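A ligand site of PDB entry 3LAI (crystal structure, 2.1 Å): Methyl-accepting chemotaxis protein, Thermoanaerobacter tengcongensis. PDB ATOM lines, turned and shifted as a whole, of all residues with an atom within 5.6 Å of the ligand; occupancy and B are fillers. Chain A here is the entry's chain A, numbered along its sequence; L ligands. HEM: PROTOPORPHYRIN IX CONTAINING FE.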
ATOM      1  N   MET A   1      34.450  -5.511  17.637  1.00  0.00           N
ATOM      2  CA  MET A   1      33.788  -6.340  18.633  1.00  0.00           C
ATOM      3  C   MET A   1      34.744  -7.271  19.348  1.00  0.00           C
ATOM      4  O   MET A   1      35.869  -7.489  18.905  1.00  0.00           O
ATOM      5  CB  MET A   1      32.697  -7.210  17.995  1.00  0.00           C
ATOM      6  CG  MET A   1      31.287  -6.738  18.261  1.00  0.00           C
ATOM      7  SD  MET A   1      30.970  -5.261  17.320  1.00  0.00           S
ATOM      8  CE  MET A   1      31.177  -5.907  15.667  1.00  0.00           C
ATOM      9  N   LYS A   2      34.291  -7.835  20.447  1.00  0.00           N
ATOM     10  CA  LYS A   2      34.962  -8.933  21.096  1.00  0.00           C
ATOM     11  C   LYS A   2      34.719 -10.246  20.351  1.00  0.00           C
ATOM     12  O   LYS A   2      33.782 -10.374  19.599  1.00  0.00           O
ATOM     13  CB  LYS A   2      34.498  -9.078  22.529  1.00  0.00           C
ATOM     14  CG  LYS A   2      34.599  -7.853  23.380  1.00  0.00           C
ATOM     15  CD  LYS A   2      36.040  -7.410  23.597  1.00  0.00           C
ATOM     16  CE  LYS A   2      36.910  -8.528  24.131  1.00  0.00           C
ATOM     17  NZ  LYS A   2      38.134  -8.012  24.717  1.00  0.00           N
ATOM     18  N   GLY A   3      35.547 -11.232  20.624  1.00  0.00           N
ATOM     19  CA  GLY A   3      35.508 -12.503  19.916  1.00  0.00           C
ATOM     20  C   GLY A   3      34.206 -13.284  20.015  1.00  0.00           C
ATOM     21  O   GLY A   3      33.766 -13.893  19.036  1.00  0.00           O
ATOM     22  N   ILE A   5      30.981 -12.566  20.116  1.00  0.00           N
ATOM     23  CA  ILE A   5      29.931 -12.232  19.188  1.00  0.00           C
ATOM     24  C   ILE A   5      30.285 -12.551  17.753  1.00  0.00           C
ATOM     25  O   ILE A   5      29.462 -12.995  17.036  1.00  0.00           O
ATOM     26  CB  ILE A   5      29.441 -10.814  19.388  1.00  0.00           C
ATOM     27  CG1 ILE A   5      28.178 -10.574  18.581  1.00  0.00           C
ATOM     28  CG2 ILE A   5      30.425  -9.864  18.955  1.00  0.00           C
ATOM     29  CD1 ILE A   5      27.331  -9.535  19.131  1.00  0.00           C
ATOM     30  N   TRP A   9      28.294 -14.853  14.766  1.00  0.00           N
ATOM     31  CA  TRP A   9      27.972 -14.367  13.419  1.00  0.00           C
ATOM     32  C   TRP A   9      28.438 -15.338  12.347  1.00  0.00           C
ATOM     33  O   TRP A   9      27.693 -15.650  11.424  1.00  0.00           O
ATOM     34  CB  TRP A   9      28.543 -12.963  13.162  1.00  0.00           C
ATOM     35  CG  TRP A   9      27.923 -11.898  14.022  1.00  0.00           C
ATOM     36  CD1 TRP A   9      26.732 -11.986  14.694  1.00  0.00           C
ATOM     37  CD2 TRP A   9      28.431 -10.593  14.291  1.00  0.00           C
ATOM     38  NE1 TRP A   9      26.492 -10.826  15.383  1.00  0.00           N
ATOM     39  CE2 TRP A   9      27.508  -9.944  15.143  1.00  0.00           C
ATOM     40  CE3 TRP A   9      29.581  -9.893  13.896  1.00  0.00           C
ATOM     41  CZ2 TRP A   9      27.702  -8.652  15.610  1.00  0.00           C
ATOM     42  CZ3 TRP A   9      29.765  -8.600  14.368  1.00  0.00           C
ATOM     43  CH2 TRP A   9      28.833  -7.989  15.206  1.00  0.00           C
ATOM     44  N   ILE A  75      19.631 -15.335  17.261  1.00  0.00           N
ATOM     45  CA  ILE A  75      18.976 -15.659  18.530  1.00  0.00           C
ATOM     46  C   ILE A  75      19.008 -17.174  18.779  1.00  0.00           C
ATOM     47  O   ILE A  75      19.218 -17.623  19.914  1.00  0.00           O
ATOM     48  CB  ILE A  75      17.501 -15.210  18.550  1.00  0.00           C
ATOM     49  CG1 ILE A  75      17.392 -13.681  18.536  1.00  0.00           C
ATOM     50  CG2 ILE A  75      16.798 -15.768  19.777  1.00  0.00           C
ATOM     51  CD1 ILE A  75      18.314 -13.009  19.535  1.00  0.00           C
ATOM     52  N   PHE A  78      22.687 -18.005  19.636  1.00  0.00           N
ATOM     53  CA  PHE A  78      23.089 -17.477  20.931  1.00  0.00           C
ATOM     54  C   PHE A  78      22.439 -18.243  22.091  1.00  0.00           C
ATOM     55  O   PHE A  78      23.058 -18.472  23.136  1.00  0.00           O
ATOM     56  CB  PHE A  78      22.724 -15.999  21.039  1.00  0.00           C
ATOM     57  CG  PHE A  78      23.599 -15.215  21.960  1.00  0.00           C
ATOM     58  CD1 PHE A  78      24.763 -14.617  21.498  1.00  0.00           C
ATOM     59  CD2 PHE A  78      23.272 -15.073  23.298  1.00  0.00           C
ATOM     60  CE1 PHE A  78      25.582 -13.900  22.344  1.00  0.00           C
ATOM     61  CE2 PHE A  78      24.098 -14.355  24.157  1.00  0.00           C
ATOM     62  CZ  PHE A  78      25.251 -13.765  23.677  1.00  0.00           C
ATOM     63  N   TYR A  85      20.291 -17.296  29.702  1.00  0.00           N
ATOM     64  CA  TYR A  85      19.612 -16.024  29.482  1.00  0.00           C
ATOM     65  C   TYR A  85      18.204 -16.226  28.964  1.00  0.00           C
ATOM     66  O   TYR A  85      17.365 -15.330  29.058  1.00  0.00           O
ATOM     67  CB  TYR A  85      20.388 -15.181  28.486  1.00  0.00           C
ATOM     68  CG  TYR A  85      21.741 -14.721  28.959  1.00  0.00           C
ATOM     69  CD1 TYR A  85      22.897 -15.380  28.581  1.00  0.00           C
ATOM     70  CD2 TYR A  85      21.853 -13.606  29.778  1.00  0.00           C
ATOM     71  CE1 TYR A  85      24.145 -14.948  29.010  1.00  0.00           C
ATOM     72  CE2 TYR A  85      23.088 -13.153  30.203  1.00  0.00           C
ATOM     73  CZ  TYR A  85      24.220 -13.827  29.824  1.00  0.00           C
ATOM     74  OH  TYR A  85      25.435 -13.381  30.253  1.00  0.00           O
ATOM     75  N   PHE A  86      17.950 -17.382  28.391  1.00  0.00           N
ATOM     76  CA  PHE A  86      16.713 -17.679  27.736  1.00  0.00           C
ATOM     77  C   PHE A  86      15.832 -18.612  28.590  1.00  0.00           C
ATOM     78  O   PHE A  86      14.899 -19.182  28.127  1.00  0.00           O
ATOM     79  CB  PHE A  86      16.993 -18.304  26.364  1.00  0.00           C
ATOM     80  CG  PHE A  86      17.713 -17.411  25.426  1.00  0.00           C
ATOM     81  CD1 PHE A  86      17.028 -16.593  24.593  1.00  0.00           C
ATOM     82  CD2 PHE A  86      19.053 -17.396  25.355  1.00  0.00           C
ATOM     83  CE1 PHE A  86      17.694 -15.769  23.733  1.00  0.00           C
ATOM     84  CE2 PHE A  86      19.677 -16.600  24.505  1.00  0.00           C
ATOM     85  CZ  PHE A  86      18.994 -15.786  23.697  1.00  0.00           C
ATOM     86  N   PHE A  94      12.499 -11.066  29.287  1.00  0.00           N
ATOM     87  CA  PHE A  94      13.731 -11.192  28.547  1.00  0.00           C
ATOM     88  C   PHE A  94      14.194  -9.863  28.034  1.00  0.00           C
ATOM     89  O   PHE A  94      15.265  -9.464  28.265  1.00  0.00           O
ATOM     90  CB  PHE A  94      13.537 -12.157  27.390  1.00  0.00           C
ATOM     91  CG  PHE A  94      14.733 -12.337  26.506  1.00  0.00           C
ATOM     92  CD1 PHE A  94      15.780 -13.133  26.870  1.00  0.00           C
ATOM     93  CD2 PHE A  94      14.767 -11.779  25.264  1.00  0.00           C
ATOM     94  CE1 PHE A  94      16.842 -13.313  26.052  1.00  0.00           C
ATOM     95  CE2 PHE A  94      15.816 -11.980  24.447  1.00  0.00           C
ATOM     96  CZ  PHE A  94      16.856 -12.737  24.834  1.00  0.00           C
ATOM     97  N   LEU A  95      13.310  -9.203  27.314  1.00  0.00           N
ATOM     98  CA  LEU A  95      13.599  -7.922  26.716  1.00  0.00           C
ATOM     99  C   LEU A  95      13.878  -6.856  27.766  1.00  0.00           C
ATOM    100  O   LEU A  95      14.732  -6.038  27.590  1.00  0.00           O
ATOM    101  CB  LEU A  95      12.445  -7.472  25.814  1.00  0.00           C
ATOM    102  CG  LEU A  95      12.100  -8.259  24.546  1.00  0.00           C
ATOM    103  CD1 LEU A  95      10.938  -7.716  23.872  1.00  0.00           C
ATOM    104  CD2 LEU A  95      13.211  -8.418  23.609  1.00  0.00           C
ATOM    105  N   MET A  98      17.522  -7.016  29.262  1.00  0.00           N
ATOM    106  CA  MET A  98      18.666  -6.999  28.365  1.00  0.00           C
ATOM    107  C   MET A  98      19.607  -5.824  28.648  1.00  0.00           C
ATOM    108  O   MET A  98      20.832  -5.961  28.571  1.00  0.00           O
ATOM    109  CB  MET A  98      18.246  -7.013  26.893  1.00  0.00           C
ATOM    110  CG  MET A  98      18.054  -8.408  26.293  1.00  0.00           C
ATOM    111  SD  MET A  98      19.323  -9.598  26.796  1.00  0.00           S
ATOM    112  CE  MET A  98      18.496 -10.502  28.104  1.00  0.00           C
ATOM    113  N   VAL A 101      21.917  -6.541  31.467  1.00  0.00           N
ATOM    114  CA  VAL A 101      22.896  -7.510  31.070  1.00  0.00           C
ATOM    115  C   VAL A 101      23.989  -6.798  30.316  1.00  0.00           C
ATOM    116  O   VAL A 101      25.133  -7.043  30.523  1.00  0.00           O
ATOM    117  CB  VAL A 101      22.275  -8.613  30.254  1.00  0.00           C
ATOM    118  CG1 VAL A 101      23.307  -9.469  29.563  1.00  0.00           C
ATOM    119  CG2 VAL A 101      21.374  -9.429  31.079  1.00  0.00           C
ATOM    120  N   LEU A 105      28.096  -6.491  31.417  1.00  0.00           N
ATOM    121  CA  LEU A 105      29.226  -6.994  30.636  1.00  0.00           C
ATOM    122  C   LEU A 105      30.275  -5.940  30.291  1.00  0.00           C
ATOM    123  O   LEU A 105      31.434  -6.239  30.173  1.00  0.00           O
ATOM    124  CB  LEU A 105      28.747  -7.669  29.362  1.00  0.00           C
ATOM    125  CG  LEU A 105      27.781  -8.830  29.472  1.00  0.00           C
ATOM    126  CD1 LEU A 105      26.979  -8.902  28.249  1.00  0.00           C
ATOM    127  CD2 LEU A 105      28.506 -10.109  29.693  1.00  0.00           C
ATOM    128  N   GLY A 111      37.004  -4.159  27.398  1.00  0.00           N
ATOM    129  CA  GLY A 111      36.780  -3.819  26.018  1.00  0.00           C
ATOM    130  C   GLY A 111      35.414  -4.100  25.439  1.00  0.00           C
ATOM    131  O   GLY A 111      35.164  -3.683  24.338  1.00  0.00           O
ATOM    132  N   ALA A 112      34.543  -4.807  26.160  1.00  0.00           N
ATOM    133  CA  ALA A 112      33.225  -5.185  25.657  1.00  0.00           C
ATOM    134  C   ALA A 112      32.352  -3.971  25.550  1.00  0.00           C
ATOM    135  O   ALA A 112      32.340  -3.164  26.427  1.00  0.00           O
ATOM    136  CB  ALA A 112      32.589  -6.171  26.530  1.00  0.00           C
ATOM    137  N   THR A 113      31.604  -3.869  24.470  1.00  0.00           N
ATOM    138  CA  THR A 113      30.926  -2.635  24.172  1.00  0.00           C
ATOM    139  C   THR A 113      29.454  -2.743  23.670  1.00  0.00           C
ATOM    140  O   THR A 113      29.069  -2.167  22.704  1.00  0.00           O
ATOM    141  CB  THR A 113      31.850  -1.822  23.262  1.00  0.00           C
ATOM    142  OG1 THR A 113      32.474  -0.817  24.033  1.00  0.00           O
ATOM    143  CG2 THR A 113      31.167  -1.222  22.164  1.00  0.00           C
ATOM    144  N   PRO A 114      28.643  -3.479  24.380  1.00  0.00           N
ATOM    145  CA  PRO A 114      27.285  -3.658  23.929  1.00  0.00           C
ATOM    146  C   PRO A 114      26.475  -2.385  24.015  1.00  0.00           C
ATOM    147  O   PRO A 114      26.708  -1.572  24.863  1.00  0.00           O
ATOM    148  CB  PRO A 114      26.747  -4.691  24.883  1.00  0.00           C
ATOM    149  CG  PRO A 114      27.538  -4.580  26.018  1.00  0.00           C
ATOM    150  CD  PRO A 114      28.873  -4.230  25.607  1.00  0.00           C
ATOM    151  N   PRO A 115      25.523  -2.246  23.123  1.00  0.00           N
ATOM    152  CA  PRO A 115      24.657  -1.075  23.075  1.00  0.00           C
ATOM    153  C   PRO A 115      23.727  -0.975  24.270  1.00  0.00           C
ATOM    154  O   PRO A 115      23.519  -1.929  24.919  1.00  0.00           O
ATOM    155  CB  PRO A 115      23.877  -1.288  21.801  1.00  0.00           C
ATOM    156  CG  PRO A 115      24.035  -2.684  21.512  1.00  0.00           C
ATOM    157  CD  PRO A 115      25.300  -3.123  21.987  1.00  0.00           C
ATOM    158  N   LEU A 117      20.087  -0.865  25.527  1.00  0.00           N
ATOM    159  CA  LEU A 117      18.779  -1.305  25.092  1.00  0.00           C
ATOM    160  C   LEU A 117      17.749  -0.905  26.132  1.00  0.00           C
ATOM    161  O   LEU A 117      17.158  -1.731  26.797  1.00  0.00           O
ATOM    162  CB  LEU A 117      18.757  -2.791  24.839  1.00  0.00           C
ATOM    163  CG  LEU A 117      19.815  -3.327  23.907  1.00  0.00           C
ATOM    164  CD1 LEU A 117      19.854  -4.806  23.872  1.00  0.00           C
ATOM    165  CD2 LEU A 117      19.638  -2.782  22.571  1.00  0.00           C
ATOM    166  N   MET A 129      11.538   0.329  23.324  1.00  0.00           N
ATOM    167  CA  MET A 129      12.923  -0.065  23.468  1.00  0.00           C
ATOM    168  C   MET A 129      13.782   0.774  22.541  1.00  0.00           C
ATOM    169  O   MET A 129      13.534   0.850  21.336  1.00  0.00           O
ATOM    170  CB  MET A 129      13.098  -1.556  23.157  1.00  0.00           C
ATOM    171  CG  MET A 129      14.552  -2.005  23.246  1.00  0.00           C
ATOM    172  SD  MET A 129      14.771  -3.794  23.176  1.00  0.00           S
ATOM    173  CE  MET A 129      14.691  -4.204  24.928  1.00  0.00           C
ATOM    174  N   TYR A 131      17.521   1.401  21.134  1.00  0.00           N
ATOM    175  CA  TYR A 131      18.881   1.001  20.830  1.00  0.00           C
ATOM    176  C   TYR A 131      19.732   2.260  20.705  1.00  0.00           C
ATOM    177  O   TYR A 131      19.357   3.211  20.010  1.00  0.00           O
ATOM    178  CB  TYR A 131      18.853   0.211  19.518  1.00  0.00           C
ATOM    179  CG  TYR A 131      20.180   0.047  18.812  1.00  0.00           C
ATOM    180  CD1 TYR A 131      21.034  -1.000  19.119  1.00  0.00           C
ATOM    181  CD2 TYR A 131      20.544   0.919  17.787  1.00  0.00           C
ATOM    182  CE1 TYR A 131      22.230  -1.168  18.445  1.00  0.00           C
ATOM    183  CE2 TYR A 131      21.738   0.767  17.128  1.00  0.00           C
ATOM    184  CZ  TYR A 131      22.578  -0.285  17.451  1.00  0.00           C
ATOM    185  OH  TYR A 131      23.774  -0.411  16.772  1.00  0.00           O
ATOM    186  N   SER A 133      23.870   3.242  20.186  1.00  0.00           N
ATOM    187  CA  SER A 133      25.186   2.748  19.918  1.00  0.00           C
ATOM    188  C   SER A 133      26.038   3.674  19.073  1.00  0.00           C
ATOM    189  O   SER A 133      25.540   4.449  18.338  1.00  0.00           O
ATOM    190  CB  SER A 133      25.042   1.374  19.256  1.00  0.00           C
ATOM    191  OG  SER A 133      26.204   0.839  18.729  1.00  0.00           O
ATOM    192  N   LYS A 134      27.340   3.555  19.243  1.00  0.00           N
ATOM    193  CA  LYS A 134      28.319   4.185  18.415  1.00  0.00           C
ATOM    194  C   LYS A 134      28.399   3.448  17.127  1.00  0.00           C
ATOM    195  O   LYS A 134      28.762   4.004  16.135  1.00  0.00           O
ATOM    196  CB  LYS A 134      29.690   4.151  19.039  1.00  0.00           C
ATOM    197  CG  LYS A 134      30.066   5.365  19.789  1.00  0.00           C
ATOM    198  CD  LYS A 134      30.010   5.143  21.269  1.00  0.00           C
ATOM    199  CE  LYS A 134      30.905   6.067  22.064  1.00  0.00           C
ATOM    200  NZ  LYS A 134      32.306   5.735  21.955  1.00  0.00           N
ATOM    201  N   ARG A 135      28.069   2.170  17.123  1.00  0.00           N
ATOM    202  CA  ARG A 135      28.032   1.386  15.921  1.00  0.00           C
ATOM    203  C   ARG A 135      26.699   1.616  15.323  1.00  0.00           C
ATOM    204  O   ARG A 135      25.934   2.372  15.824  1.00  0.00           O
ATOM    205  CB  ARG A 135      28.251  -0.086  16.216  1.00  0.00           C
ATOM    206  CG  ARG A 135      29.556  -0.355  16.850  1.00  0.00           C
ATOM    207  CD  ARG A 135      29.985  -1.760  16.706  1.00  0.00           C
ATOM    208  NE  ARG A 135      31.244  -1.979  17.334  1.00  0.00           N
ATOM    209  CZ  ARG A 135      31.372  -2.219  18.609  1.00  0.00           C
ATOM    210  NH1 ARG A 135      30.332  -2.289  19.367  1.00  0.00           N
ATOM    211  NH2 ARG A 135      32.558  -2.404  19.119  1.00  0.00           N
ATOM    212  N   LYS A 136      26.382   1.002  14.237  1.00  0.00           N
ATOM    213  CA  LYS A 136      25.073   1.292  13.781  1.00  0.00           C
ATOM    214  C   LYS A 136      24.462   0.076  13.144  1.00  0.00           C
ATOM    215  O   LYS A 136      24.621  -0.131  11.988  1.00  0.00           O
ATOM    216  CB  LYS A 136      25.130   2.464  12.829  1.00  0.00           C
ATOM    217  CG  LYS A 136      23.844   2.778  12.268  1.00  0.00           C
ATOM    218  CD  LYS A 136      23.858   4.062  11.707  1.00  0.00           C
ATOM    219  CE  LYS A 136      24.189   4.013  10.323  1.00  0.00           C
ATOM    220  NZ  LYS A 136      24.908   5.210  10.108  1.00  0.00           N
ATOM    221  N   MET A 137      23.791  -0.721  13.930  1.00  0.00           N
ATOM    222  CA  MET A 137      23.320  -1.993  13.475  1.00  0.00           C
ATOM    223  C   MET A 137      21.821  -2.064  13.615  1.00  0.00           C
ATOM    224  O   MET A 137      21.296  -2.914  14.255  1.00  0.00           O
ATOM    225  CB  MET A 137      24.075  -3.150  14.158  1.00  0.00           C
ATOM    226  CG  MET A 137      25.558  -2.872  14.365  1.00  0.00           C
ATOM    227  SD  MET A 137      26.716  -4.085  14.917  1.00  0.00           S
ATOM    228  CE  MET A 137      26.380  -5.358  13.868  1.00  0.00           C
ATOM    229  N   TYR A 140      20.223  -5.343  12.371  1.00  0.00           N
ATOM    230  CA  TYR A 140      20.593  -6.465  13.245  1.00  0.00           C
ATOM    231  C   TYR A 140      19.695  -6.423  14.487  1.00  0.00           C
ATOM    232  O   TYR A 140      19.082  -7.422  14.853  1.00  0.00           O
ATOM    233  CB  TYR A 140      22.071  -6.357  13.631  1.00  0.00           C
ATOM    234  CG  TYR A 140      22.591  -7.530  14.429  1.00  0.00           C
ATOM    235  CD1 TYR A 140      22.434  -8.842  13.969  1.00  0.00           C
ATOM    236  CD2 TYR A 140      23.255  -7.325  15.637  1.00  0.00           C
ATOM    237  CE1 TYR A 140      22.919  -9.924  14.694  1.00  0.00           C
ATOM    238  CE2 TYR A 140      23.742  -8.397  16.384  1.00  0.00           C
ATOM    239  CZ  TYR A 140      23.566  -9.691  15.908  1.00  0.00           C
ATOM    240  OH  TYR A 140      24.042 -10.758  16.635  1.00  0.00           O
ATOM    241  N   PHE A 141      19.619  -5.257  15.101  1.00  0.00           N
ATOM    242  CA  PHE A 141      18.777  -5.013  16.253  1.00  0.00           C
ATOM    243  C   PHE A 141      17.340  -5.460  16.002  1.00  0.00           C
ATOM    244  O   PHE A 141      16.787  -6.234  16.794  1.00  0.00           O
ATOM    245  CB  PHE A 141      18.795  -3.529  16.605  1.00  0.00           C
ATOM    246  CG  PHE A 141      17.757  -3.126  17.609  1.00  0.00           C
ATOM    247  CD1 PHE A 141      17.752  -3.681  18.884  1.00  0.00           C
ATOM    248  CD2 PHE A 141      16.806  -2.166  17.301  1.00  0.00           C
ATOM    249  CE1 PHE A 141      16.809  -3.293  19.813  1.00  0.00           C
ATOM    250  CE2 PHE A 141      15.851  -1.773  18.228  1.00  0.00           C
ATOM    251  CZ  PHE A 141      15.845  -2.337  19.480  1.00  0.00           C
ATOM    252  N   LEU A 144      17.071  -9.202  15.777  1.00  0.00           N
ATOM    253  CA  LEU A 144      17.165  -9.842  17.097  1.00  0.00           C
ATOM    254  C   LEU A 144      15.817  -9.849  17.805  1.00  0.00           C
ATOM    255  O   LEU A 144      15.435 -10.816  18.470  1.00  0.00           O
ATOM    256  CB  LEU A 144      18.215  -9.138  17.949  1.00  0.00           C
ATOM    257  CG  LEU A 144      19.642  -9.246  17.401  1.00  0.00           C
ATOM    258  CD1 LEU A 144      20.607  -8.398  18.207  1.00  0.00           C
ATOM    259  CD2 LEU A 144      20.103 -10.697  17.342  1.00  0.00           C
ATOM    260  N   ILE A 145      15.087  -8.746  17.657  1.00  0.00           N
ATOM    261  CA  ILE A 145      13.785  -8.644  18.269  1.00  0.00           C
ATOM    262  C   ILE A 145      12.870  -9.731  17.708  1.00  0.00           C
ATOM    263  O   ILE A 145      12.237 -10.467  18.474  1.00  0.00           O
ATOM    264  CB  ILE A 145      13.172  -7.235  18.051  1.00  0.00           C
ATOM    265  CG1 ILE A 145      13.920  -6.210  18.921  1.00  0.00           C
ATOM    266  CG2 ILE A 145      11.702  -7.246  18.387  1.00  0.00           C
ATOM    267  CD1 ILE A 145      13.612  -4.778  18.591  1.00  0.00           C
ATOM    268  N   SER A 148      13.831 -13.125  18.898  1.00  0.00           N
ATOM    269  CA  SER A 148      13.431 -13.333  20.288  1.00  0.00           C
ATOM    270  C   SER A 148      11.961 -13.748  20.352  1.00  0.00           C
ATOM    271  O   SER A 148      11.612 -14.729  21.017  1.00  0.00           O
ATOM    272  CB  SER A 148      13.659 -12.055  21.095  1.00  0.00           C
ATOM    273  OG  SER A 148      15.039 -11.713  21.082  1.00  0.00           O
HETATM  274  CHA HEM L   1      26.190  -6.893  20.959  1.00  0.00           C
HETATM  275  CHB HEM L   1      25.462  -9.473  24.999  1.00  0.00           C
HETATM  276  CHC HEM L   1      20.928 -10.301  23.630  1.00  0.00           C
HETATM  277  CHD HEM L   1      21.384  -6.261  21.029  1.00  0.00           C
HETATM  278  C1A HEM L   1      26.407  -7.626  22.095  1.00  0.00           C
HETATM  279  C2A HEM L   1      27.709  -7.979  22.628  1.00  0.00           C
HETATM  280  C3A HEM L   1      27.520  -8.696  23.748  1.00  0.00           C
HETATM  281  C4A HEM L   1      26.091  -8.807  23.961  1.00  0.00           C
HETATM  282  CMA HEM L   1      28.628  -9.290  24.645  1.00  0.00           C
HETATM  283  CAA HEM L   1      29.045  -7.597  21.960  1.00  0.00           C
HETATM  284  CBA HEM L   1      29.792  -6.537  22.762  1.00  0.00           C
HETATM  285  CGA HEM L   1      31.163  -6.450  22.130  1.00  0.00           C
HETATM  286  O1A HEM L   1      31.830  -5.401  22.279  1.00  0.00           O
HETATM  287  O2A HEM L   1      31.559  -7.443  21.456  1.00  0.00           O
HETATM  288  C1B HEM L   1      24.215 -10.044  24.945  1.00  0.00           C
HETATM  289  C2B HEM L   1      23.693 -11.146  25.745  1.00  0.00           C
HETATM  290  C3B HEM L   1      22.444 -11.374  25.355  1.00  0.00           C
HETATM  291  C4B HEM L   1      22.109 -10.422  24.313  1.00  0.00           C
HETATM  292  CMB HEM L   1      24.427 -11.943  26.856  1.00  0.00           C
HETATM  293  CAB HEM L   1      21.507 -12.441  25.932  1.00  0.00           C
HETATM  294  CBB HEM L   1      20.551 -12.963  25.168  1.00  0.00           C
HETATM  295  C1C HEM L   1      20.614  -9.211  22.843  1.00  0.00           C
HETATM  296  C2C HEM L   1      19.292  -8.830  22.375  1.00  0.00           C
HETATM  297  C3C HEM L   1      19.425  -7.731  21.634  1.00  0.00           C
HETATM  298  C4C HEM L   1      20.821  -7.349  21.647  1.00  0.00           C
HETATM  299  CMC HEM L   1      17.978  -9.589  22.640  1.00  0.00           C
HETATM  300  CAC HEM L   1      18.325  -6.892  20.936  1.00  0.00           C
HETATM  301  CBC HEM L   1      17.071  -6.900  21.397  1.00  0.00           C
HETATM  302  C1D HEM L   1      22.678  -6.171  20.592  1.00  0.00           C
HETATM  303  C2D HEM L   1      23.123  -5.504  19.403  1.00  0.00           C
HETATM  304  C3D HEM L   1      24.644  -5.682  19.372  1.00  0.00           C
HETATM  305  C4D HEM L   1      24.947  -6.468  20.548  1.00  0.00           C
HETATM  306  CMD HEM L   1      22.217  -4.772  18.402  1.00  0.00           C
HETATM  307  CAD HEM L   1      25.611  -5.177  18.282  1.00  0.00           C
HETATM  308  CBD HEM L   1      26.571  -4.138  18.848  1.00  0.00           C
HETATM  309  CGD HEM L   1      26.031  -2.749  18.536  1.00  0.00           C
HETATM  310  O1D HEM L   1      26.654  -1.773  19.011  1.00  0.00           O
HETATM  311  O2D HEM L   1      24.988  -2.608  17.832  1.00  0.00           O
HETATM  312  NA  HEM L   1      25.440  -8.141  22.934  1.00  0.00           N
HETATM  313  NB  HEM L   1      23.211  -9.644  24.096  1.00  0.00           N
HETATM  314  NC  HEM L   1      21.515  -8.286  22.385  1.00  0.00           N
HETATM  315  ND  HEM L   1      23.775  -6.726  21.231  1.00  0.00           N
HETATM  316 FE   HEM L   1      23.430  -8.155  22.649  1.00  0.00          FE
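The side-chain sulfur of Met 137 lies close to an oxygen (O2D) of the ligand (3.7 Å).
Met 1 touches the ligand (CG to O2A, 3.3 Å).
Ile 5 touches the ligand.
Phe 78 touches the ligand.
Tyr 85 touches the ligand.
Phe 86 touches the ligand (CZ to CBB, 3.5 Å).
Phe 94 touches the ligand (CE2 to CMC, 3.7 Å).
Met 98 touches the ligand (SD to CHC, 3.6 Å).
Val 101 touches the ligand.
Leu 105 touches the ligand.
C of Ala 112 touches O1A of the ligand, 3.6 Å away.
Pro 114 touches the ligand.
Pro 115 touches the ligand (CD to CBD, 3.5 Å).
Leu 117 touches the ligand (CD1 to C4C, 3.5 Å).
CD2 of Tyr 140 touches CMD of the ligand, at 3.9 Å.
Phe 141 touches the ligand (CD1 to CAC, 3.9 Å).
Leu 144 touches the ligand.
Ser 148 touches the ligand (OG to CMC, 3.9 Å).
Within 4 Å of the ligand: Met 1, Lys 2, Ile 5, Phe 78, Tyr 85, Phe 86, Phe 94, Met 98, Val 101, Leu 105, Ala 112, Thr 113, Pro 114, Pro 115, Leu 117, Tyr 131, Ser 133, Arg 135, Met 137, Tyr 140, Phe 141, Leu 144 and Ser 148.
The nearest printed residue that does not touch the ligand is Ile 145 (4.1 Å).
SD of Met 1 sits at hydrogen-bond distance from NE of Arg 135.
The side-chain hydroxyl (OH) of Tyr 131 lies close to the side-chain hydroxyl (OG) of Ser 133 (3.4 Å).
The side-chain hydroxyl (OH) of Tyr 140 lies within hydrogen-bond range of the indole nitrogen (NE1) of Trp 9 (2.8 Å).
The side-chain hydroxyl (OH) of Tyr 131 lies within hydrogen-bond range of the backbone NH (N) of Met 137 (2.9 Å).
The side-chain hydroxyl of Ser 148 lies within hydrogen-bond range of the backbone carbonyl oxygen of Leu 144, at 2.8 Å.
The side-chain hydroxyl (OG) of Ser 133 sits at hydrogen-bond distance from the backbone NH (N) of Arg 135 (2.8 Å).
The side-chain hydroxyl (OG) of Ser 133 is in hydrogen-bond range of an oxygen (O1D) of the ligand (2.7 Å).
N of Thr 113 sits at hydrogen-bond distance from O1A of the ligand.
The side-chain hydroxyl (OH) of Tyr 131 sits at hydrogen-bond distance from an oxygen (O2D) of the ligand (2.7 Å).
NH1 of Arg 135 is in salt-bridge range of O1D of the ligand (3.7 Å).
An oxygen (O2A) of the ligand sits at hydrogen-bond distance from the backbone NH (N) of Lys 2.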
